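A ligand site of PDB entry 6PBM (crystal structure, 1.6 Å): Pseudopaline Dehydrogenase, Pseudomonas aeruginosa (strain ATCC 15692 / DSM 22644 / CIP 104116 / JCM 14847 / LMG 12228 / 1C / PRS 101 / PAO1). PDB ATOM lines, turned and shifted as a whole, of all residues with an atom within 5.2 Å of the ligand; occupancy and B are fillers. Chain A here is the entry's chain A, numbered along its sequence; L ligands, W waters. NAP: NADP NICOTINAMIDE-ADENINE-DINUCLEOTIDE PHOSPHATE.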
ATOM      1  N   GLY A  31      14.544 -21.597  -5.138  1.00  0.00           N
ATOM      2  CA  GLY A  31      13.823 -21.489  -6.385  1.00  0.00           C
ATOM      3  C   GLY A  31      14.855 -21.485  -7.492  1.00  0.00           C
ATOM      4  O   GLY A  31      15.856 -20.775  -7.371  1.00  0.00           O
ATOM      5  N   LEU A  32      14.694 -22.281  -8.517  1.00  0.00           N
ATOM      6  CA  LEU A  32      15.678 -22.322  -9.611  1.00  0.00           C
ATOM      7  C   LEU A  32      14.938 -22.255 -10.936  1.00  0.00           C
ATOM      8  O   LEU A  32      14.834 -23.233 -11.683  1.00  0.00           O
ATOM      9  CB  LEU A  32      16.583 -23.581  -9.506  1.00  0.00           C
ATOM     10  CG  LEU A  32      17.673 -23.694 -10.560  1.00  0.00           C
ATOM     11  CD1 LEU A  32      18.592 -22.527 -10.491  1.00  0.00           C
ATOM     12  CD2 LEU A  32      18.492 -24.945 -10.363  1.00  0.00           C
ATOM     13  N   GLY A  33      14.384 -21.073 -11.214  1.00  0.00           N
ATOM     14  CA  GLY A  33      13.763 -20.753 -12.470  1.00  0.00           C
ATOM     15  C   GLY A  33      14.536 -19.677 -13.229  1.00  0.00           C
ATOM     16  O   GLY A  33      15.763 -19.578 -13.083  1.00  0.00           O
ATOM     17  N   ALA A  34      13.806 -18.893 -14.012  1.00  0.00           N
ATOM     18  CA  ALA A  34      14.417 -17.930 -14.937  1.00  0.00           C
ATOM     19  C   ALA A  34      15.235 -16.888 -14.177  1.00  0.00           C
ATOM     20  O   ALA A  34      16.402 -16.625 -14.514  1.00  0.00           O
ATOM     21  CB  ALA A  34      13.331 -17.245 -15.750  1.00  0.00           C
ATOM     22  N   VAL A  35      14.655 -16.300 -13.127  1.00  0.00           N
ATOM     23  CA  VAL A  35      15.357 -15.289 -12.332  1.00  0.00           C
ATOM     24  C   VAL A  35      16.626 -15.887 -11.737  1.00  0.00           C
ATOM     25  O   VAL A  35      17.700 -15.270 -11.746  1.00  0.00           O
ATOM     26  CB  VAL A  35      14.426 -14.755 -11.225  1.00  0.00           C
ATOM     27  CG1 VAL A  35      15.197 -14.094 -10.121  1.00  0.00           C
ATOM     28  CG2 VAL A  35      13.381 -13.840 -11.805  1.00  0.00           C
ATOM     29  N   ALA A  36      16.530 -17.106 -11.203  1.00  0.00           N
ATOM     30  CA  ALA A  36      17.675 -17.709 -10.544  1.00  0.00           C
ATOM     31  C   ALA A  36      18.848 -17.888 -11.501  1.00  0.00           C
ATOM     32  O   ALA A  36      19.994 -17.831 -11.079  1.00  0.00           O
ATOM     33  CB  ALA A  36      17.256 -19.069  -9.977  1.00  0.00           C
ATOM     34  N   ASN A  55      14.969 -26.387  -4.785  1.00  0.00           N
ATOM     35  CA  ASN A  55      13.692 -26.226  -5.469  1.00  0.00           C
ATOM     36  C   ASN A  55      12.775 -27.369  -5.050  1.00  0.00           C
ATOM     37  O   ASN A  55      13.206 -28.525  -4.998  1.00  0.00           O
ATOM     38  CB  ASN A  55      13.827 -26.230  -6.984  1.00  0.00           C
ATOM     39  CG  ASN A  55      12.645 -25.609  -7.670  1.00  0.00           C
ATOM     40  OD1 ASN A  55      12.406 -24.435  -7.504  1.00  0.00           O
ATOM     41  ND2 ASN A  55      11.872 -26.399  -8.410  1.00  0.00           N
ATOM     42  N   HIS A  56      11.522 -27.035  -4.726  1.00  0.00           N
ATOM     43  CA  HIS A  56      10.616 -28.052  -4.197  1.00  0.00           C
ATOM     44  C   HIS A  56      10.359 -29.138  -5.236  1.00  0.00           C
ATOM     45  O   HIS A  56      10.531 -28.938  -6.441  1.00  0.00           O
ATOM     46  CB  HIS A  56       9.325 -27.402  -3.687  1.00  0.00           C
ATOM     47  CG  HIS A  56       8.490 -26.712  -4.705  1.00  0.00           C
ATOM     48  ND1 HIS A  56       7.249 -26.181  -4.390  1.00  0.00           N
ATOM     49  CD2 HIS A  56       8.691 -26.433  -6.015  1.00  0.00           C
ATOM     50  CE1 HIS A  56       6.721 -25.629  -5.470  1.00  0.00           C
ATOM     51  NE2 HIS A  56       7.583 -25.750  -6.473  1.00  0.00           N
ATOM     52  N   PRO A  57       9.961 -30.332  -4.785  1.00  0.00           N
ATOM     53  CA  PRO A  57       9.764 -31.445  -5.726  1.00  0.00           C
ATOM     54  C   PRO A  57       8.723 -31.161  -6.783  1.00  0.00           C
ATOM     55  O   PRO A  57       7.761 -30.420  -6.576  1.00  0.00           O
ATOM     56  CB  PRO A  57       9.331 -32.603  -4.807  1.00  0.00           C
ATOM     57  CG  PRO A  57       9.708 -32.223  -3.469  1.00  0.00           C
ATOM     58  CD  PRO A  57       9.857 -30.752  -3.374  1.00  0.00           C
ATOM     59  N   GLY A  58       8.935 -31.775  -7.932  1.00  0.00           N
ATOM     60  CA  GLY A  58       8.039 -31.585  -9.041  1.00  0.00           C
ATOM     61  C   GLY A  58       8.762 -31.890 -10.332  1.00  0.00           C
ATOM     62  O   GLY A  58       9.921 -32.300 -10.340  1.00  0.00           O
ATOM     63  N   ARG A  60       9.781 -29.918 -12.710  1.00  0.00           N
ATOM     64  CA  ARG A  60      10.954 -29.083 -12.983  1.00  0.00           C
ATOM     65  C   ARG A  60      12.169 -29.578 -12.222  1.00  0.00           C
ATOM     66  O   ARG A  60      13.249 -29.700 -12.788  1.00  0.00           O
ATOM     67  CB  ARG A  60      10.662 -27.612 -12.646  1.00  0.00           C
ATOM     68  CG  ARG A  60      11.790 -26.667 -13.099  1.00  0.00           C
ATOM     69  CD  ARG A  60      11.683 -25.255 -12.517  1.00  0.00           C
ATOM     70  NE  ARG A  60      10.401 -24.588 -12.749  1.00  0.00           N
ATOM     71  CZ  ARG A  60      10.177 -23.611 -13.642  1.00  0.00           C
ATOM     72  NH1 ARG A  60      11.151 -23.166 -14.433  1.00  0.00           N
ATOM     73  NH2 ARG A  60       8.967 -23.074 -13.722  1.00  0.00           N
ATOM     74  N   SER A  61      12.010 -29.857 -10.913  1.00  0.00           N
ATOM     75  CA  SER A  61      13.134 -30.330 -10.117  1.00  0.00           C
ATOM     76  C   SER A  61      13.663 -31.654 -10.642  1.00  0.00           C
ATOM     77  O   SER A  61      14.875 -31.900 -10.575  1.00  0.00           O
ATOM     78  CB  SER A  61      12.749 -30.494  -8.648  1.00  0.00           C
ATOM     79  OG  SER A  61      12.748 -29.219  -8.034  1.00  0.00           O
ATOM     80  N   CYS A 111      14.385 -16.688  -5.164  1.00  0.00           N
ATOM     81  CA  CYS A 111      14.062 -16.544  -6.574  1.00  0.00           C
ATOM     82  C   CYS A 111      12.709 -17.167  -6.889  1.00  0.00           C
ATOM     83  O   CYS A 111      12.329 -17.308  -8.059  1.00  0.00           O
ATOM     84  CB  CYS A 111      15.156 -17.196  -7.416  1.00  0.00           C
ATOM     85  SG  CYS A 111      16.822 -16.435  -7.133  1.00  0.00           S
ATOM     86  N   VAL A 112      11.972 -17.572  -5.871  1.00  0.00           N
ATOM     87  CA  VAL A 112      10.608 -18.063  -6.006  1.00  0.00           C
ATOM     88  C   VAL A 112       9.678 -16.889  -6.276  1.00  0.00           C
ATOM     89  O   VAL A 112      10.048 -15.715  -6.070  1.00  0.00           O
ATOM     90  CB  VAL A 112      10.203 -18.821  -4.737  1.00  0.00           C
ATOM     91  CG1 VAL A 112      11.067 -20.050  -4.547  1.00  0.00           C
ATOM     92  CG2 VAL A 112      10.268 -17.891  -3.518  1.00  0.00           C
ATOM     93  N   PRO A 113       8.454 -17.157  -6.696  1.00  0.00           N
ATOM     94  CA  PRO A 113       7.479 -16.076  -6.840  1.00  0.00           C
ATOM     95  C   PRO A 113       7.283 -15.313  -5.532  1.00  0.00           C
ATOM     96  O   PRO A 113       7.251 -15.888  -4.444  1.00  0.00           O
ATOM     97  CB  PRO A 113       6.193 -16.809  -7.258  1.00  0.00           C
ATOM     98  CG  PRO A 113       6.702 -18.099  -7.888  1.00  0.00           C
ATOM     99  CD  PRO A 113       7.881 -18.482  -7.019  1.00  0.00           C
ATOM    100  N   ALA A 114       7.134 -13.991  -5.652  1.00  0.00           N
ATOM    101  CA  ALA A 114       6.960 -13.166  -4.477  1.00  0.00           C
ATOM    102  C   ALA A 114       5.717 -13.526  -3.661  1.00  0.00           C
ATOM    103  O   ALA A 114       5.709 -13.354  -2.440  1.00  0.00           O
ATOM    104  CB  ALA A 114       6.921 -11.689  -4.912  1.00  0.00           C
ATOM    105  N   SER A 116       4.894 -16.387  -2.863  1.00  0.00           N
ATOM    106  CA  SER A 116       5.223 -17.594  -2.133  1.00  0.00           C
ATOM    107  C   SER A 116       6.243 -17.351  -1.034  1.00  0.00           C
ATOM    108  O   SER A 116       6.669 -18.302  -0.367  1.00  0.00           O
ATOM    109  CB  SER A 116       5.756 -18.690  -3.069  1.00  0.00           C
ATOM    110  OG  SER A 116       7.075 -18.442  -3.513  1.00  0.00           O
ATOM    111  N   VAL A 120       7.607 -20.151   1.618  1.00  0.00           N
ATOM    112  CA  VAL A 120       8.944 -20.653   1.373  1.00  0.00           C
ATOM    113  C   VAL A 120       9.825 -20.405   2.579  1.00  0.00           C
ATOM    114  O   VAL A 120      10.574 -21.277   3.006  1.00  0.00           O
ATOM    115  CB  VAL A 120       9.497 -20.033   0.079  1.00  0.00           C
ATOM    116  CG1 VAL A 120      10.980 -20.269  -0.032  1.00  0.00           C
ATOM    117  CG2 VAL A 120       8.782 -20.636  -1.144  1.00  0.00           C
ATOM    118  N   SER A 139      12.266  -9.907  -5.770  1.00  0.00           N
ATOM    119  CA  SER A 139      11.113  -9.147  -6.283  1.00  0.00           C
ATOM    120  C   SER A 139      10.224  -8.780  -5.095  1.00  0.00           C
ATOM    121  O   SER A 139       9.165  -9.378  -4.853  1.00  0.00           O
ATOM    122  CB  SER A 139      10.369  -9.957  -7.341  1.00  0.00           C
ATOM    123  OG  SER A 139       9.139  -9.324  -7.652  1.00  0.00           O
ATOM    124  N   TYR A 166      12.673  -7.370  -9.856  1.00  0.00           N
ATOM    125  CA  TYR A 166      13.629  -8.120 -10.665  1.00  0.00           C
ATOM    126  C   TYR A 166      14.179  -7.194 -11.753  1.00  0.00           C
ATOM    127  O   TYR A 166      13.431  -6.421 -12.338  1.00  0.00           O
ATOM    128  CB  TYR A 166      12.994  -9.344 -11.289  1.00  0.00           C
ATOM    129  CG  TYR A 166      13.964 -10.103 -12.154  1.00  0.00           C
ATOM    130  CD1 TYR A 166      15.187 -10.520 -11.668  1.00  0.00           C
ATOM    131  CD2 TYR A 166      13.659 -10.379 -13.469  1.00  0.00           C
ATOM    132  CE1 TYR A 166      16.070 -11.204 -12.460  1.00  0.00           C
ATOM    133  CE2 TYR A 166      14.545 -11.069 -14.269  1.00  0.00           C
ATOM    134  CZ  TYR A 166      15.749 -11.463 -13.767  1.00  0.00           C
ATOM    135  OH  TYR A 166      16.644 -12.151 -14.567  1.00  0.00           O
ATOM    136  N   ALA A 168      15.531  -7.540 -14.795  1.00  0.00           N
ATOM    137  CA  ALA A 168      15.572  -7.911 -16.198  1.00  0.00           C
ATOM    138  C   ALA A 168      14.231  -8.506 -16.605  1.00  0.00           C
ATOM    139  O   ALA A 168      13.254  -8.482 -15.851  1.00  0.00           O
ATOM    140  CB  ALA A 168      16.747  -8.859 -16.433  1.00  0.00           C
ATOM    141  N   ALA A 169      14.173  -8.965 -17.848  1.00  0.00           N
ATOM    142  CA  ALA A 169      13.105  -9.821 -18.326  1.00  0.00           C
ATOM    143  C   ALA A 169      13.775 -11.093 -18.829  1.00  0.00           C
ATOM    144  O   ALA A 169      14.565 -11.052 -19.779  1.00  0.00           O
ATOM    145  CB  ALA A 169      12.285  -9.175 -19.438  1.00  0.00           C
ATOM    146  N   THR A 170      13.435 -12.206 -18.199  1.00  0.00           N
ATOM    147  CA  THR A 170      14.133 -13.470 -18.412  1.00  0.00           C
ATOM    148  C   THR A 170      13.108 -14.598 -18.438  1.00  0.00           C
ATOM    149  O   THR A 170      12.163 -14.610 -17.642  1.00  0.00           O
ATOM    150  CB  THR A 170      15.146 -13.734 -17.284  1.00  0.00           C
ATOM    151  OG1 THR A 170      15.991 -12.601 -17.123  1.00  0.00           O
ATOM    152  CG2 THR A 170      16.018 -14.949 -17.560  1.00  0.00           C
ATOM    153  N   LYS A 171      13.308 -15.541 -19.362  1.00  0.00           N
ATOM    154  CA  LYS A 171      12.397 -16.667 -19.508  1.00  0.00           C
ATOM    155  C   LYS A 171      13.184 -17.945 -19.764  1.00  0.00           C
ATOM    156  O   LYS A 171      14.231 -17.927 -20.426  1.00  0.00           O
ATOM    157  CB  LYS A 171      11.425 -16.433 -20.665  1.00  0.00           C
ATOM    158  CG  LYS A 171      10.294 -17.394 -20.694  1.00  0.00           C
ATOM    159  CD  LYS A 171       9.187 -16.972 -21.633  1.00  0.00           C
ATOM    160  CE  LYS A 171       8.057 -18.002 -21.571  1.00  0.00           C
ATOM    161  NZ  LYS A 171       8.057 -18.744 -20.254  1.00  0.00           N
ATOM    162  N   VAL A 172      12.695 -19.052 -19.211  1.00  0.00           N
ATOM    163  CA  VAL A 172      13.192 -20.376 -19.581  1.00  0.00           C
ATOM    164  C   VAL A 172      12.511 -20.720 -20.903  1.00  0.00           C
ATOM    165  O   VAL A 172      11.300 -20.904 -20.967  1.00  0.00           O
ATOM    166  CB  VAL A 172      12.911 -21.416 -18.489  1.00  0.00           C
ATOM    167  CG1 VAL A 172      13.240 -22.805 -18.987  1.00  0.00           C
ATOM    168  CG2 VAL A 172      13.763 -21.111 -17.275  1.00  0.00           C
ATOM    169  N   THR A 231       6.033  -3.916 -10.851  1.00  0.00           N
ATOM    170  CA  THR A 231       4.856  -4.697 -11.220  1.00  0.00           C
ATOM    171  C   THR A 231       3.650  -4.318 -10.371  1.00  0.00           C
ATOM    172  O   THR A 231       2.520  -4.353 -10.863  1.00  0.00           O
ATOM    173  CB  THR A 231       5.143  -6.189 -11.141  1.00  0.00           C
ATOM    174  OG1 THR A 231       5.784  -6.538  -9.921  1.00  0.00           O
ATOM    175  CG2 THR A 231       6.088  -6.569 -12.272  1.00  0.00           C
ATOM    176  N   ARG A 376       0.745 -16.816 -13.491  1.00  0.00           N
ATOM    177  CA  ARG A 376       1.295 -15.889 -12.499  1.00  0.00           C
ATOM    178  C   ARG A 376       0.758 -14.466 -12.686  1.00  0.00           C
ATOM    179  O   ARG A 376       0.392 -13.793 -11.705  1.00  0.00           O
ATOM    180  CB  ARG A 376       2.812 -15.907 -12.590  1.00  0.00           C
ATOM    181  CG  ARG A 376       3.482 -15.159 -11.498  1.00  0.00           C
ATOM    182  CD  ARG A 376       4.880 -15.729 -11.250  1.00  0.00           C
ATOM    183  NE  ARG A 376       4.803 -17.139 -10.841  1.00  0.00           N
ATOM    184  CZ  ARG A 376       5.650 -18.075 -11.251  1.00  0.00           C
ATOM    185  NH1 ARG A 376       6.642 -17.751 -12.066  1.00  0.00           N
ATOM    186  NH2 ARG A 376       5.500 -19.322 -10.830  1.00  0.00           N
ATOM    187  N   GLU A 380      -0.361 -13.842  -8.959  1.00  0.00           N
ATOM    188  CA  GLU A 380       0.620 -13.211  -8.083  1.00  0.00           C
ATOM    189  C   GLU A 380       0.277 -11.745  -7.880  1.00  0.00           C
ATOM    190  O   GLU A 380       0.407 -11.214  -6.763  1.00  0.00           O
ATOM    191  CB  GLU A 380       2.023 -13.357  -8.658  1.00  0.00           C
ATOM    192  CG  GLU A 380       3.100 -12.567  -7.856  1.00  0.00           C
ATOM    193  CD  GLU A 380       4.555 -12.877  -8.308  1.00  0.00           C
ATOM    194  OE1 GLU A 380       4.751 -13.673  -9.243  1.00  0.00           O
ATOM    195  OE2 GLU A 380       5.503 -12.301  -7.738  1.00  0.00           O
HETATM  196  PA  NAP L   1       9.924 -19.346 -12.630  1.00  0.00           P
HETATM  197  O1A NAP L   1      10.797 -19.463 -13.882  1.00  0.00           O
HETATM  198  O2A NAP L   1       8.523 -19.886 -12.745  1.00  0.00           O
HETATM  199  O5B NAP L   1      10.805 -19.952 -11.398  1.00  0.00           O
HETATM  200  C5B NAP L   1      10.199 -19.981 -10.116  1.00  0.00           C
HETATM  201  C4B NAP L   1      10.952 -21.069  -9.327  1.00  0.00           C
HETATM  202  O4B NAP L   1      10.450 -21.159  -8.096  1.00  0.00           O
HETATM  203  C3B NAP L   1      10.740 -22.401 -10.047  1.00  0.00           C
HETATM  204  O3B NAP L   1      11.862 -23.189  -9.945  1.00  0.00           O
HETATM  205  C2B NAP L   1       9.560 -22.957  -9.215  1.00  0.00           C
HETATM  206  O2B NAP L   1       9.572 -24.442  -9.332  1.00  0.00           O
HETATM  207  C1B NAP L   1       9.671 -22.533  -7.939  1.00  0.00           C
HETATM  208  N9A NAP L   1       8.344 -22.200  -7.387  1.00  0.00           N
HETATM  209  C8A NAP L   1       7.244 -21.704  -7.936  1.00  0.00           C
HETATM  210  N7A NAP L   1       6.261 -21.598  -7.024  1.00  0.00           N
HETATM  211  C5A NAP L   1       6.764 -22.040  -5.870  1.00  0.00           C
HETATM  212  C6A NAP L   1       6.203 -22.143  -4.619  1.00  0.00           C
HETATM  213  N6A NAP L   1       4.853 -21.797  -4.251  1.00  0.00           N
HETATM  214  N1A NAP L   1       6.930 -22.659  -3.609  1.00  0.00           N
HETATM  215  C2A NAP L   1       8.213 -23.024  -3.801  1.00  0.00           C
HETATM  216  N3A NAP L   1       8.772 -22.885  -5.044  1.00  0.00           N
HETATM  217  C4A NAP L   1       8.056 -22.402  -6.076  1.00  0.00           C
HETATM  218  O3  NAP L   1       9.611 -17.812 -12.108  1.00  0.00           O
HETATM  219  PN  NAP L   1      10.588 -16.525 -12.459  1.00  0.00           P
HETATM  220  O1N NAP L   1      11.990 -16.977 -12.165  1.00  0.00           O
HETATM  221  O2N NAP L   1      10.319 -16.155 -13.906  1.00  0.00           O
HETATM  222  O5D NAP L   1      10.015 -15.369 -11.451  1.00  0.00           O
HETATM  223  C5D NAP L   1      10.223 -15.416 -10.066  1.00  0.00           C
HETATM  224  C4D NAP L   1       9.687 -14.073  -9.477  1.00  0.00           C
HETATM  225  O4D NAP L   1      10.257 -13.020 -10.109  1.00  0.00           O
HETATM  226  C3D NAP L   1       8.158 -13.918  -9.665  1.00  0.00           C
HETATM  227  O3D NAP L   1       7.643 -13.205  -8.612  1.00  0.00           O
HETATM  228  C2D NAP L   1       8.121 -12.961 -10.842  1.00  0.00           C
HETATM  229  O2D NAP L   1       6.743 -12.359 -10.949  1.00  0.00           O
HETATM  230  C1D NAP L   1       9.090 -12.087 -10.590  1.00  0.00           C
HETATM  231  N1N NAP L   1       9.462 -11.459 -11.848  1.00  0.00           N
HETATM  232  C2N NAP L   1      10.082 -12.169 -12.845  1.00  0.00           C
HETATM  233  C3N NAP L   1      10.331 -11.551 -14.046  1.00  0.00           C
HETATM  234  C7N NAP L   1      11.034 -12.291 -15.172  1.00  0.00           C
HETATM  235  O7N NAP L   1      11.429 -11.707 -16.148  1.00  0.00           O
HETATM  236  N7N NAP L   1      11.272 -13.696 -15.061  1.00  0.00           N
HETATM  237  C4N NAP L   1       9.977 -10.241 -14.230  1.00  0.00           C
HETATM  238  C5N NAP L   1       9.373  -9.548 -13.226  1.00  0.00           C
HETATM  239  C6N NAP L   1       9.088 -10.185 -12.032  1.00  0.00           C
HETATM  240  P2B NAP L   1       8.204 -25.146  -9.883  1.00  0.00           P
HETATM  241  O1X NAP L   1       7.942 -24.635 -11.248  1.00  0.00           O
HETATM  242  O2X NAP L   1       8.521 -26.636  -9.797  1.00  0.00           O
HETATM  243  O3X NAP L   1       7.128 -24.781  -8.901  1.00  0.00           O
HETATM  244  O   HOH W   1       7.385 -15.222 -13.566  1.00  0.00           O
HETATM  245  O   HOH W   2       6.929 -21.622 -11.342  1.00  0.00           O
HETATM  246  O   HOH W   3       7.112 -26.150 -13.308  1.00  0.00           O
HETATM  247  O   HOH W   4       3.670 -22.537  -1.585  1.00  0.00           O
HETATM  248  O   HOH W   5       6.172 -23.610  -1.057  1.00  0.00           O
HETATM  249  O   HOH W   6      13.754 -18.318 -10.411  1.00  0.00           O
HETATM  250  O   HOH W   7       7.461 -28.286 -11.774  1.00  0.00           O
HETATM  251  O   HOH W   8       5.114 -11.961 -12.983  1.00  0.00           O
HETATM  252  O   HOH W   9       9.335 -16.888 -16.234  1.00  0.00           O
HETATM  253  O   HOH W  10      10.265 -20.958 -15.914  1.00  0.00           O
HETATM  254  O   HOH W  11       9.287  -7.416  -9.951  1.00  0.00           O
HETATM  255  O   HOH W  12       6.581 -28.274  -8.389  1.00  0.00           O
HETATM  256  O   HOH W  13       9.759 -28.944  -9.254  1.00  0.00           O
HETATM  257  O   HOH W  14      10.415  -6.439 -12.695  1.00  0.00           O
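An oxygen (O2A) of the ligand lies within salt-bridge range of the guanidinium group of Arg 376. N of Ala 34 lies within hydrogen-bond range of O1A of the ligand, at 3.1 Å. O3B of the ligand lies close to O of Leu 32, 3.4 Å away. An oxygen (O3X) of the ligand lies within hydrogen-bond range of a ring nitrogen (NE2) of His 56, 2.7 Å away. The backbone NH (N) of Leu 32 is in hydrogen-bond range of an oxygen (O3B) of the ligand, 3.3 Å away. An oxygen (O3D) of the ligand is in hydrogen-bond range of the side-chain carboxylate (OE2) of Glu 380, 2.5 Å away. An oxygen (O1N) of the ligand sits at hydrogen-bond distance from the backbone NH (N) of Val 35 (2.9 Å). O3B of the ligand is in hydrogen-bond range of OD1 of Asn 55 (2.8 Å). O of Thr 170 lies within hydrogen-bond range of N7N of the ligand. N of Thr 170 sits at hydrogen-bond distance from O7N of the ligand (2.9 Å). The backbone NH (N) of Ala 114 lies within hydrogen-bond range of an oxygen (O3D) of the ligand (3.1 Å). O1X of the ligand is in salt-bridge range of NE of Arg 60 (2.9 Å).
The side-chain hydroxyl of Thr 170 sits at hydrogen-bond distance from the side-chain hydroxyl of Tyr 166. The side-chain hydroxyl of Ser 61 sits at hydrogen-bond distance from the side-chain amide nitrogen of Asn 55. The side-chain hydroxyl (OG) of Ser 116 lies within hydrogen-bond range of the backbone carbonyl oxygen (O) of Pro 113, 2.7 Å away. The side-chain amide oxygen of Asn 55 sits at hydrogen-bond distance from the backbone NH of Leu 32, 3.3 Å away. The side-chain hydroxyl (OG) of Ser 61 lies within hydrogen-bond range of the backbone carbonyl oxygen (O) of His 56, at 2.7 Å. The side-chain carboxylate of Glu 380 sits at hydrogen-bond distance from the backbone NH of Ala 114, 3.1 Å away. The guanidinium group (NE) of Arg 376 is in salt-bridge range of the side-chain carboxylate (OE1) of Glu 380.
Residues that only touch the ligand: Gly 31 (3.8 Å), Gly 33 (3.2 Å), Cys 111 (3.5 Å), Val 112 (3.7 Å), Pro 113 (3.4 Å), Ser 116 (3.4 Å), Val 120 (3.6 Å), Tyr 166 (3.6 Å), Ala 168 (3.7 Å) and Ala 169 (3.3 Å). Hydrophobic or aromatic side chains that line the ligand: Ala 34, Val 35, His 56, Val 112, Pro 113, Val 120 and Tyr 166. 20 residues have an atom within 4 Å of the ligand: Gly 31, Leu 32, Gly 33, Ala 34, Val 35, Asn 55, His 56, Arg 60, Cys 111, Val 112, Pro 113, Ala 114, Ser 116, Val 120, Tyr 166, Ala 168, Ala 169, Thr 170, Arg 376 and Glu 380.
Water W2 lies within hydrogen-bond range of an oxygen (O2A) of the ligand (2.7 Å), the guanidinium group of Arg 376 (2.8 Å) and the guanidinium group of Arg 60 (3.5 Å). Water W7 lies within hydrogen-bond range of an oxygen (O2X) of the ligand (2.8 Å) and the backbone NH (N) of Arg 60 (3.0 Å). Water W6 lies within hydrogen-bond range of O1N of the ligand (2.8 Å), O of Cys 111 (2.9 Å), N of Gly 33 (2.9 Å) and N of Ala 36 (3.1 Å). Water W12 lies within hydrogen-bond range of an oxygen (O2X) of the ligand (2.9 Å), the backbone carbonyl oxygen of Pro 57 (3.0 Å) and a ring nitrogen (NE2) of His 56 (3.3 Å). Water W1 lies within hydrogen-bond range of NH1 of Arg 376 (3.0 Å) and O2N of the ligand (3.1 Å). Water W11 bridges the side-chain hydroxyl of Ser 139 (3.0 Å) and the backbone NH of Tyr 166 (3.4 Å).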
